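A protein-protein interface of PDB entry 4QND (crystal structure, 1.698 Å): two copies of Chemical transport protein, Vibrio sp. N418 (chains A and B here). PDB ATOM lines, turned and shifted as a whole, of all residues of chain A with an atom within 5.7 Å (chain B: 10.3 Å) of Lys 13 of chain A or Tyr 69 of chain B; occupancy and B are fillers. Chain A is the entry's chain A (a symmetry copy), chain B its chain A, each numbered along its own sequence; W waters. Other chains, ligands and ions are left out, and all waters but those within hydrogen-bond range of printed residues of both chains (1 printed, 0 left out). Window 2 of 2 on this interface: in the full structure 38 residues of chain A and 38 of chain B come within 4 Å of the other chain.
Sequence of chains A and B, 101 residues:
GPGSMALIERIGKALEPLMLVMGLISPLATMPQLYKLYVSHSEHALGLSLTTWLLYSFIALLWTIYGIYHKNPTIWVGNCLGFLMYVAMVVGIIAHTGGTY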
ATOM      1  N   ILE A   8      15.935  -4.129 -19.600  1.00  0.00           N
ATOM      2  CA  ILE A   8      16.539  -4.953 -18.562  1.00  0.00           C
ATOM      3  C   ILE A   8      16.466  -4.258 -17.202  1.00  0.00           C
ATOM      4  O   ILE A   8      16.127  -4.880 -16.195  1.00  0.00           O
ATOM      5  CB  ILE A   8      18.001  -5.292 -18.909  1.00  0.00           C
ATOM      6  CG1 ILE A   8      18.038  -6.277 -20.080  1.00  0.00           C
ATOM      7  CG2 ILE A   8      18.731  -5.868 -17.702  1.00  0.00           C
ATOM      8  CD1 ILE A   8      19.431  -6.662 -20.522  1.00  0.00           C
ATOM      9  N   GLU A   9      16.760  -2.961 -17.179  1.00  0.00           N
ATOM     10  CA  GLU A   9      16.665  -2.194 -15.942  1.00  0.00           C
ATOM     11  C   GLU A   9      15.232  -2.136 -15.420  1.00  0.00           C
ATOM     12  O   GLU A   9      14.990  -2.332 -14.231  1.00  0.00           O
ATOM     13  CB  GLU A   9      17.192  -0.774 -16.142  1.00  0.00           C
ATOM     14  CG  GLU A   9      16.908   0.121 -14.953  1.00  0.00           C
ATOM     15  CD  GLU A   9      17.207   1.574 -15.233  1.00  0.00           C
ATOM     16  OE1 GLU A   9      17.938   1.855 -16.203  1.00  0.00           O
ATOM     17  OE2 GLU A   9      16.704   2.437 -14.485  1.00  0.00           O
ATOM     18  N   ARG A  10      14.290  -1.858 -16.318  1.00  0.00           N
ATOM     19  CA  ARG A  10      12.882  -1.738 -15.953  1.00  0.00           C
ATOM     20  C   ARG A  10      12.378  -3.014 -15.286  1.00  0.00           C
ATOM     21  O   ARG A  10      11.733  -2.969 -14.239  1.00  0.00           O
ATOM     22  CB  ARG A  10      12.035  -1.424 -17.188  1.00  0.00           C
ATOM     23  CG  ARG A  10      10.590  -1.039 -16.897  1.00  0.00           C
ATOM     24  CD  ARG A  10      10.468   0.442 -16.559  1.00  0.00           C
ATOM     25  NE  ARG A  10       9.122   0.950 -16.814  1.00  0.00           N
ATOM     26  CZ  ARG A  10       8.161   1.022 -15.899  1.00  0.00           C
ATOM     27  NH1 ARG A  10       8.391   0.618 -14.657  1.00  0.00           N
ATOM     28  NH2 ARG A  10       6.969   1.500 -16.225  1.00  0.00           N
ATOM     29  N   ILE A  11      12.685  -4.153 -15.898  1.00  0.00           N
ATOM     30  CA  ILE A  11      12.272  -5.441 -15.355  1.00  0.00           C
ATOM     31  C   ILE A  11      13.013  -5.739 -14.053  1.00  0.00           C
ATOM     32  O   ILE A  11      12.403  -6.138 -13.065  1.00  0.00           O
ATOM     33  CB  ILE A  11      12.506  -6.576 -16.370  1.00  0.00           C
ATOM     34  CG1 ILE A  11      11.658  -6.339 -17.623  1.00  0.00           C
ATOM     35  CG2 ILE A  11      12.172  -7.923 -15.750  1.00  0.00           C
ATOM     36  CD1 ILE A  11      11.917  -7.326 -18.745  1.00  0.00           C
ATOM     37  N   GLY A  12      14.327  -5.524 -14.055  1.00  0.00           N
ATOM     38  CA  GLY A  12      15.150  -5.765 -12.881  1.00  0.00           C
ATOM     39  C   GLY A  12      14.668  -5.019 -11.651  1.00  0.00           C
ATOM     40  O   GLY A  12      14.591  -5.580 -10.557  1.00  0.00           O
ATOM     41  N   LYS A  13      14.330  -3.748 -11.832  1.00  0.00           N
ATOM     42  CA  LYS A  13      13.833  -2.939 -10.726  1.00  0.00           C
ATOM     43  C   LYS A  13      12.436  -3.370 -10.284  1.00  0.00           C
ATOM     44  O   LYS A  13      12.132  -3.376  -9.093  1.00  0.00           O
ATOM     45  CB  LYS A  13      13.821  -1.461 -11.115  1.00  0.00           C
ATOM     46  CG  LYS A  13      15.183  -0.795 -11.059  1.00  0.00           C
ATOM     47  CD  LYS A  13      15.068   0.671 -11.424  1.00  0.00           C
ATOM     48  CE  LYS A  13      16.370   1.413 -11.197  1.00  0.00           C
ATOM     49  NZ  LYS A  13      16.261   2.818 -11.677  1.00  0.00           N
ATOM     50  N   ALA A  14      11.591  -3.729 -11.245  1.00  0.00           N
ATOM     51  CA  ALA A  14      10.212  -4.109 -10.949  1.00  0.00           C
ATOM     52  C   ALA A  14      10.138  -5.393 -10.128  1.00  0.00           C
ATOM     53  O   ALA A  14       9.214  -5.579  -9.339  1.00  0.00           O
ATOM     54  CB  ALA A  14       9.418  -4.266 -12.239  1.00  0.00           C
ATOM     55  N   LEU A  15      11.118  -6.270 -10.312  1.00  0.00           N
ATOM     56  CA  LEU A  15      11.136  -7.560  -9.626  1.00  0.00           C
ATOM     57  C   LEU A  15      11.544  -7.444  -8.159  1.00  0.00           C
ATOM     58  O   LEU A  15      11.265  -8.342  -7.368  1.00  0.00           O
ATOM     59  CB  LEU A  15      12.084  -8.527 -10.339  1.00  0.00           C
ATOM     60  CG  LEU A  15      11.675  -8.961 -11.747  1.00  0.00           C
ATOM     61  CD1 LEU A  15      12.741  -9.856 -12.360  1.00  0.00           C
ATOM     62  CD2 LEU A  15      10.330  -9.668 -11.722  1.00  0.00           C
ATOM     63  N   GLU A  16      12.200  -6.341  -7.803  1.00  0.00           N
ATOM     64  CA  GLU A  16      12.777  -6.187  -6.467  1.00  0.00           C
ATOM     65  C   GLU A  16      11.787  -6.461  -5.319  1.00  0.00           C
ATOM     66  O   GLU A  16      12.092  -7.256  -4.429  1.00  0.00           O
ATOM     67  CB  GLU A  16      13.393  -4.789  -6.311  1.00  0.00           C
ATOM     68  CG  GLU A  16      14.176  -4.599  -5.021  1.00  0.00           C
ATOM     69  CD  GLU A  16      15.396  -5.499  -4.933  1.00  0.00           C
ATOM     70  OE1 GLU A  16      15.814  -5.828  -3.802  1.00  0.00           O
ATOM     71  OE2 GLU A  16      15.943  -5.872  -5.992  1.00  0.00           O
ATOM     72  N   PRO A  17      10.594  -5.830  -5.333  1.00  0.00           N
ATOM     73  CA  PRO A  17       9.698  -6.143  -4.213  1.00  0.00           C
ATOM     74  C   PRO A  17       8.950  -7.467  -4.376  1.00  0.00           C
ATOM     75  O   PRO A  17       8.179  -7.840  -3.496  1.00  0.00           O
ATOM     76  CB  PRO A  17       8.712  -4.977  -4.231  1.00  0.00           C
ATOM     77  CG  PRO A  17       8.621  -4.615  -5.669  1.00  0.00           C
ATOM     78  CD  PRO A  17      10.003  -4.821  -6.233  1.00  0.00           C
ATOM     79  N   LEU B  61      13.927 -16.970 -16.713  1.00  0.00           N
ATOM     80  CA  LEU B  61      14.192 -15.796 -17.537  1.00  0.00           C
ATOM     81  C   LEU B  61      14.220 -14.523 -16.692  1.00  0.00           C
ATOM     82  O   LEU B  61      15.094 -13.675 -16.864  1.00  0.00           O
ATOM     83  CB  LEU B  61      13.144 -15.668 -18.643  1.00  0.00           C
ATOM     84  CG  LEU B  61      13.281 -14.454 -19.566  1.00  0.00           C
ATOM     85  CD1 LEU B  61      14.642 -14.443 -20.250  1.00  0.00           C
ATOM     86  CD2 LEU B  61      12.158 -14.419 -20.590  1.00  0.00           C
ATOM     87  N   LEU B  62      13.262 -14.398 -15.781  1.00  0.00           N
ATOM     88  CA  LEU B  62      13.174 -13.217 -14.928  1.00  0.00           C
ATOM     89  C   LEU B  62      14.402 -13.093 -14.028  1.00  0.00           C
ATOM     90  O   LEU B  62      14.967 -12.008 -13.892  1.00  0.00           O
ATOM     91  CB  LEU B  62      11.897 -13.251 -14.086  1.00  0.00           C
ATOM     92  CG  LEU B  62      10.575 -13.107 -14.849  1.00  0.00           C
ATOM     93  CD1 LEU B  62       9.393 -13.129 -13.892  1.00  0.00           C
ATOM     94  CD2 LEU B  62      10.568 -11.831 -15.676  1.00  0.00           C
ATOM     95  N   TRP B  63      14.819 -14.202 -13.420  1.00  0.00           N
ATOM     96  CA  TRP B  63      16.018 -14.188 -12.586  1.00  0.00           C
ATOM     97  C   TRP B  63      17.268 -13.891 -13.412  1.00  0.00           C
ATOM     98  O   TRP B  63      18.192 -13.238 -12.930  1.00  0.00           O
ATOM     99  CB  TRP B  63      16.189 -15.519 -11.848  1.00  0.00           C
ATOM    100  CG  TRP B  63      15.380 -15.631 -10.591  1.00  0.00           C
ATOM    101  CD1 TRP B  63      14.430 -16.570 -10.310  1.00  0.00           C
ATOM    102  CD2 TRP B  63      15.452 -14.779  -9.440  1.00  0.00           C
ATOM    103  NE1 TRP B  63      13.908 -16.356  -9.059  1.00  0.00           N
ATOM    104  CE2 TRP B  63      14.517 -15.262  -8.504  1.00  0.00           C
ATOM    105  CE3 TRP B  63      16.215 -13.654  -9.111  1.00  0.00           C
ATOM    106  CZ2 TRP B  63      14.323 -14.660  -7.261  1.00  0.00           C
ATOM    107  CZ3 TRP B  63      16.022 -13.056  -7.877  1.00  0.00           C
ATOM    108  CH2 TRP B  63      15.084 -13.560  -6.968  1.00  0.00           C
ATOM    109  N   THR B  64      17.299 -14.377 -14.649  1.00  0.00           N
ATOM    110  CA  THR B  64      18.430 -14.112 -15.531  1.00  0.00           C
ATOM    111  C   THR B  64      18.541 -12.613 -15.796  1.00  0.00           C
ATOM    112  O   THR B  64      19.620 -12.031 -15.691  1.00  0.00           O
ATOM    113  CB  THR B  64      18.308 -14.864 -16.871  1.00  0.00           C
ATOM    114  OG1 THR B  64      18.221 -16.275 -16.632  1.00  0.00           O
ATOM    115  CG2 THR B  64      19.520 -14.581 -17.750  1.00  0.00           C
ATOM    116  N   ILE B  65      17.414 -11.991 -16.125  1.00  0.00           N
ATOM    117  CA  ILE B  65      17.381 -10.554 -16.367  1.00  0.00           C
ATOM    118  C   ILE B  65      17.780  -9.785 -15.108  1.00  0.00           C
ATOM    119  O   ILE B  65      18.559  -8.835 -15.175  1.00  0.00           O
ATOM    120  CB  ILE B  65      15.990 -10.100 -16.844  1.00  0.00           C
ATOM    121  CG1 ILE B  65      15.703 -10.674 -18.233  1.00  0.00           C
ATOM    122  CG2 ILE B  65      15.903  -8.575 -16.878  1.00  0.00           C
ATOM    123  CD1 ILE B  65      14.254 -10.553 -18.672  1.00  0.00           C
ATOM    124  N   TYR B  66      17.256 -10.214 -13.962  1.00  0.00           N
ATOM    125  CA  TYR B  66      17.595  -9.594 -12.684  1.00  0.00           C
ATOM    126  C   TYR B  66      19.097  -9.673 -12.414  1.00  0.00           C
ATOM    127  O   TYR B  66      19.720  -8.679 -12.050  1.00  0.00           O
ATOM    128  CB  TYR B  66      16.817 -10.259 -11.542  1.00  0.00           C
ATOM    129  CG  TYR B  66      17.067  -9.639 -10.180  1.00  0.00           C
ATOM    130  CD1 TYR B  66      18.094 -10.097  -9.363  1.00  0.00           C
ATOM    131  CD2 TYR B  66      16.269  -8.605  -9.709  1.00  0.00           C
ATOM    132  CE1 TYR B  66      18.327  -9.536  -8.121  1.00  0.00           C
ATOM    133  CE2 TYR B  66      16.494  -8.036  -8.462  1.00  0.00           C
ATOM    134  CZ  TYR B  66      17.523  -8.508  -7.675  1.00  0.00           C
ATOM    135  OH  TYR B  66      17.757  -7.950  -6.435  1.00  0.00           O
ATOM    136  N   GLY B  67      19.670 -10.858 -12.597  1.00  0.00           N
ATOM    137  CA  GLY B  67      21.082 -11.071 -12.331  1.00  0.00           C
ATOM    138  C   GLY B  67      21.992 -10.317 -13.283  1.00  0.00           C
ATOM    139  O   GLY B  67      23.034  -9.795 -12.879  1.00  0.00           O
ATOM    140  N   ILE B  68      21.604 -10.268 -14.554  1.00  0.00           N
ATOM    141  CA  ILE B  68      22.355  -9.519 -15.554  1.00  0.00           C
ATOM    142  C   ILE B  68      22.348  -8.033 -15.203  1.00  0.00           C
ATOM    143  O   ILE B  68      23.385  -7.369 -15.244  1.00  0.00           O
ATOM    144  CB  ILE B  68      21.777  -9.730 -16.967  1.00  0.00           C
ATOM    145  CG1 ILE B  68      22.156 -11.120 -17.483  1.00  0.00           C
ATOM    146  CG2 ILE B  68      22.281  -8.661 -17.926  1.00  0.00           C
ATOM    147  CD1 ILE B  68      21.490 -11.495 -18.789  1.00  0.00           C
ATOM    148  N   TYR B  69      21.175  -7.524 -14.841  1.00  0.00           N
ATOM    149  CA  TYR B  69      21.031  -6.119 -14.478  1.00  0.00           C
ATOM    150  C   TYR B  69      21.936  -5.733 -13.307  1.00  0.00           C
ATOM    151  O   TYR B  69      22.567  -4.676 -13.326  1.00  0.00           O
ATOM    152  CB  TYR B  69      19.572  -5.800 -14.143  1.00  0.00           C
ATOM    153  CG  TYR B  69      19.387  -4.413 -13.571  1.00  0.00           C
ATOM    154  CD1 TYR B  69      19.764  -3.293 -14.296  1.00  0.00           C
ATOM    155  CD2 TYR B  69      18.837  -4.226 -12.313  1.00  0.00           C
ATOM    156  CE1 TYR B  69      19.605  -2.017 -13.780  1.00  0.00           C
ATOM    157  CE2 TYR B  69      18.671  -2.955 -11.785  1.00  0.00           C
ATOM    158  CZ  TYR B  69      19.056  -1.856 -12.525  1.00  0.00           C
ATOM    159  OH  TYR B  69      18.894  -0.591 -12.009  1.00  0.00           O
ATOM    160  N   HIS B  70      22.010  -6.594 -12.298  1.00  0.00           N
ATOM    161  CA  HIS B  70      22.805  -6.292 -11.111  1.00  0.00           C
ATOM    162  C   HIS B  70      24.223  -6.848 -11.176  1.00  0.00           C
ATOM    163  O   HIS B  70      24.915  -6.866 -10.163  1.00  0.00           O
ATOM    164  CB  HIS B  70      22.115  -6.823  -9.850  1.00  0.00           C
ATOM    165  CG  HIS B  70      20.957  -5.991  -9.398  1.00  0.00           C
ATOM    166  ND1 HIS B  70      19.663  -6.462  -9.385  1.00  0.00           N
ATOM    167  CD2 HIS B  70      20.898  -4.717  -8.944  1.00  0.00           C
ATOM    168  CE1 HIS B  70      18.857  -5.515  -8.940  1.00  0.00           C
ATOM    169  NE2 HIS B  70      19.581  -4.445  -8.668  1.00  0.00           N
ATOM    170  N   LYS B  71      24.645  -7.291 -12.360  1.00  0.00           N
ATOM    171  CA  LYS B  71      25.982  -7.862 -12.555  1.00  0.00           C
ATOM    172  C   LYS B  71      26.293  -8.928 -11.509  1.00  0.00           C
ATOM    173  O   LYS B  71      27.342  -8.897 -10.867  1.00  0.00           O
ATOM    174  CB  LYS B  71      27.052  -6.768 -12.510  1.00  0.00           C
ATOM    175  CG  LYS B  71      26.921  -5.724 -13.601  1.00  0.00           C
ATOM    176  CD  LYS B  71      27.090  -6.340 -14.978  1.00  0.00           C
ATOM    177  CE  LYS B  71      26.934  -5.287 -16.059  1.00  0.00           C
ATOM    178  NZ  LYS B  71      27.634  -4.028 -15.695  1.00  0.00           N
ATOM    179  N   ASN B  72      25.362  -9.857 -11.331  1.00  0.00           N
ATOM    180  CA  ASN B  72      25.486 -10.894 -10.321  1.00  0.00           C
ATOM    181  C   ASN B  72      25.429 -12.270 -10.971  1.00  0.00           C
ATOM    182  O   ASN B  72      24.350 -12.840 -11.111  1.00  0.00           O
ATOM    183  CB  ASN B  72      24.377 -10.747  -9.274  1.00  0.00           C
ATOM    184  CG  ASN B  72      24.560 -11.669  -8.076  1.00  0.00           C
ATOM    185  OD1 ASN B  72      25.179 -12.727  -8.173  1.00  0.00           O
ATOM    186  ND2 ASN B  72      24.003 -11.271  -6.939  1.00  0.00           N
ATOM    187  N   PRO B  73      26.594 -12.803 -11.376  1.00  0.00           N
ATOM    188  CA  PRO B  73      26.657 -14.102 -12.059  1.00  0.00           C
ATOM    189  C   PRO B  73      26.187 -15.264 -11.193  1.00  0.00           C
ATOM    190  O   PRO B  73      25.763 -16.278 -11.737  1.00  0.00           O
ATOM    191  CB  PRO B  73      28.146 -14.253 -12.401  1.00  0.00           C
ATOM    192  CG  PRO B  73      28.850 -13.350 -11.452  1.00  0.00           C
ATOM    193  CD  PRO B  73      27.925 -12.188 -11.250  1.00  0.00           C
ATOM    194  N   ILE B  75      23.575 -15.319  -9.653  1.00  0.00           N
ATOM    195  CA  ILE B  75      22.171 -15.408 -10.026  1.00  0.00           C
ATOM    196  C   ILE B  75      21.956 -15.761 -11.500  1.00  0.00           C
ATOM    197  O   ILE B  75      21.278 -16.742 -11.802  1.00  0.00           O
ATOM    198  CB  ILE B  75      21.427 -14.091  -9.722  1.00  0.00           C
ATOM    199  CG1 ILE B  75      21.391 -13.839  -8.213  1.00  0.00           C
ATOM    200  CG2 ILE B  75      20.014 -14.137 -10.281  1.00  0.00           C
ATOM    201  CD1 ILE B  75      20.628 -12.584  -7.818  1.00  0.00           C
ATOM    202  N   TRP B  76      22.518 -14.982 -12.425  1.00  0.00           N
ATOM    203  CA  TRP B  76      22.107 -15.127 -13.824  1.00  0.00           C
ATOM    204  C   TRP B  76      22.750 -16.301 -14.562  1.00  0.00           C
ATOM    205  O   TRP B  76      22.163 -16.814 -15.508  1.00  0.00           O
ATOM    206  CB  TRP B  76      22.351 -13.829 -14.611  1.00  0.00           C
ATOM    207  CG  TRP B  76      23.785 -13.476 -14.936  1.00  0.00           C
ATOM    208  CD1 TRP B  76      24.560 -12.550 -14.298  1.00  0.00           C
ATOM    209  CD2 TRP B  76      24.589 -13.994 -16.012  1.00  0.00           C
ATOM    210  NE1 TRP B  76      25.798 -12.477 -14.890  1.00  0.00           N
ATOM    211  CE2 TRP B  76      25.843 -13.353 -15.942  1.00  0.00           C
ATOM    212  CE3 TRP B  76      24.374 -14.944 -17.016  1.00  0.00           C
ATOM    213  CZ2 TRP B  76      26.877 -13.632 -16.835  1.00  0.00           C
ATOM    214  CZ3 TRP B  76      25.403 -15.224 -17.902  1.00  0.00           C
ATOM    215  CH2 TRP B  76      26.638 -14.570 -17.806  1.00  0.00           C
ATOM    216  N   VAL B  77      23.937 -16.731 -14.147  1.00  0.00           N
ATOM    217  CA  VAL B  77      24.602 -17.835 -14.838  1.00  0.00           C
ATOM    218  C   VAL B  77      23.769 -19.116 -14.769  1.00  0.00           C
ATOM    219  O   VAL B  77      23.430 -19.699 -15.798  1.00  0.00           O
ATOM    220  CB  VAL B  77      26.010 -18.093 -14.263  1.00  0.00           C
ATOM    221  CG1 VAL B  77      26.519 -19.456 -14.681  1.00  0.00           C
ATOM    222  CG2 VAL B  77      26.968 -16.999 -14.715  1.00  0.00           C
HETATM  223  O   HOH W   1      16.111  -4.638  -8.506  1.00  0.00           O
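The side-chain carboxylate (OE2) of Glu 16 of chain A sits at hydrogen-bond distance from the side-chain hydroxyl (OH) of Tyr 66 of chain B (2.8 Å).
NZ of Lys 13 of chain A is in salt-bridge range of OE2 of Glu 9 of chain A, 2.9 Å away.
A ring nitrogen (ND1) of His 70 of chain B lies close to the backbone carbonyl oxygen of Tyr 66 of chain B, 3.5 Å away.
Among the printed residues, merely in contact across the chains: Ile 8 of chain A with Ile 65 of chain B (3.8 Å), Ile 8 of chain A with Tyr 69 of chain B (3.7 Å), Glu 9 of chain A with Tyr 69 of chain B (3.6 Å), Ile 11 of chain A with Ile 65 of chain B (3.95 Å), Gly 12 of chain A with Tyr 66 of chain B (3.6 Å), Lys 13 of chain A with Tyr 69 of chain B (3.3 Å) and Leu 15 of chain A with Leu 62 of chain B (3.5 Å).
Lys 13 of chain A touches one residue of chain B.
Of the printed residues of chain A, Tyr 69 of chain B touches Ile 8, Glu 9 and Lys 13.
Of the printed residues of chain B, Glu 9 of chain A touches Tyr 69.
Gly 12 of chain A touches just one residue of chain B: Tyr 66 (3.6 Å).
No residue of chain B comes within 4 Å of Ala 14 of chain A.
Of the printed residues of chain B, Ile 8 of chain A touches Ile 65 (3.8 Å) and Tyr 69 (3.7 Å).
Of the printed residues of chain A, Tyr 66 of chain B touches Gly 12 and Glu 16.
Of the printed residues of chain B, Ile 11 of chain A touches Ile 65.
Printed residues of chain B within 4 Å of Glu 16 of chain A: Tyr 66.
Val 77 of chain B touches none of the printed residues of chain A.
The nearest printed residue of chain B that does not touch Glu 16 of chain A is His 70 of chain B (4.2 Å).
Of the 10 printed residues of chain A, 7 touch a printed residue of chain B.
Of the 16 printed residues of chain B, 4 touch a printed residue of chain A.
Among the printed residues, no Asp or Glu carboxylate lies within 4 Å of a Lys or Arg side-chain nitrogen of the other chain.
No position is printed for both chains.
Water W1 lies within hydrogen-bond range of O of Gly 12 of chain A (2.7 Å), OE2 of Glu 16 of chain A (2.8 Å) and NE2 of His 70 of chain B (3.5 Å).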
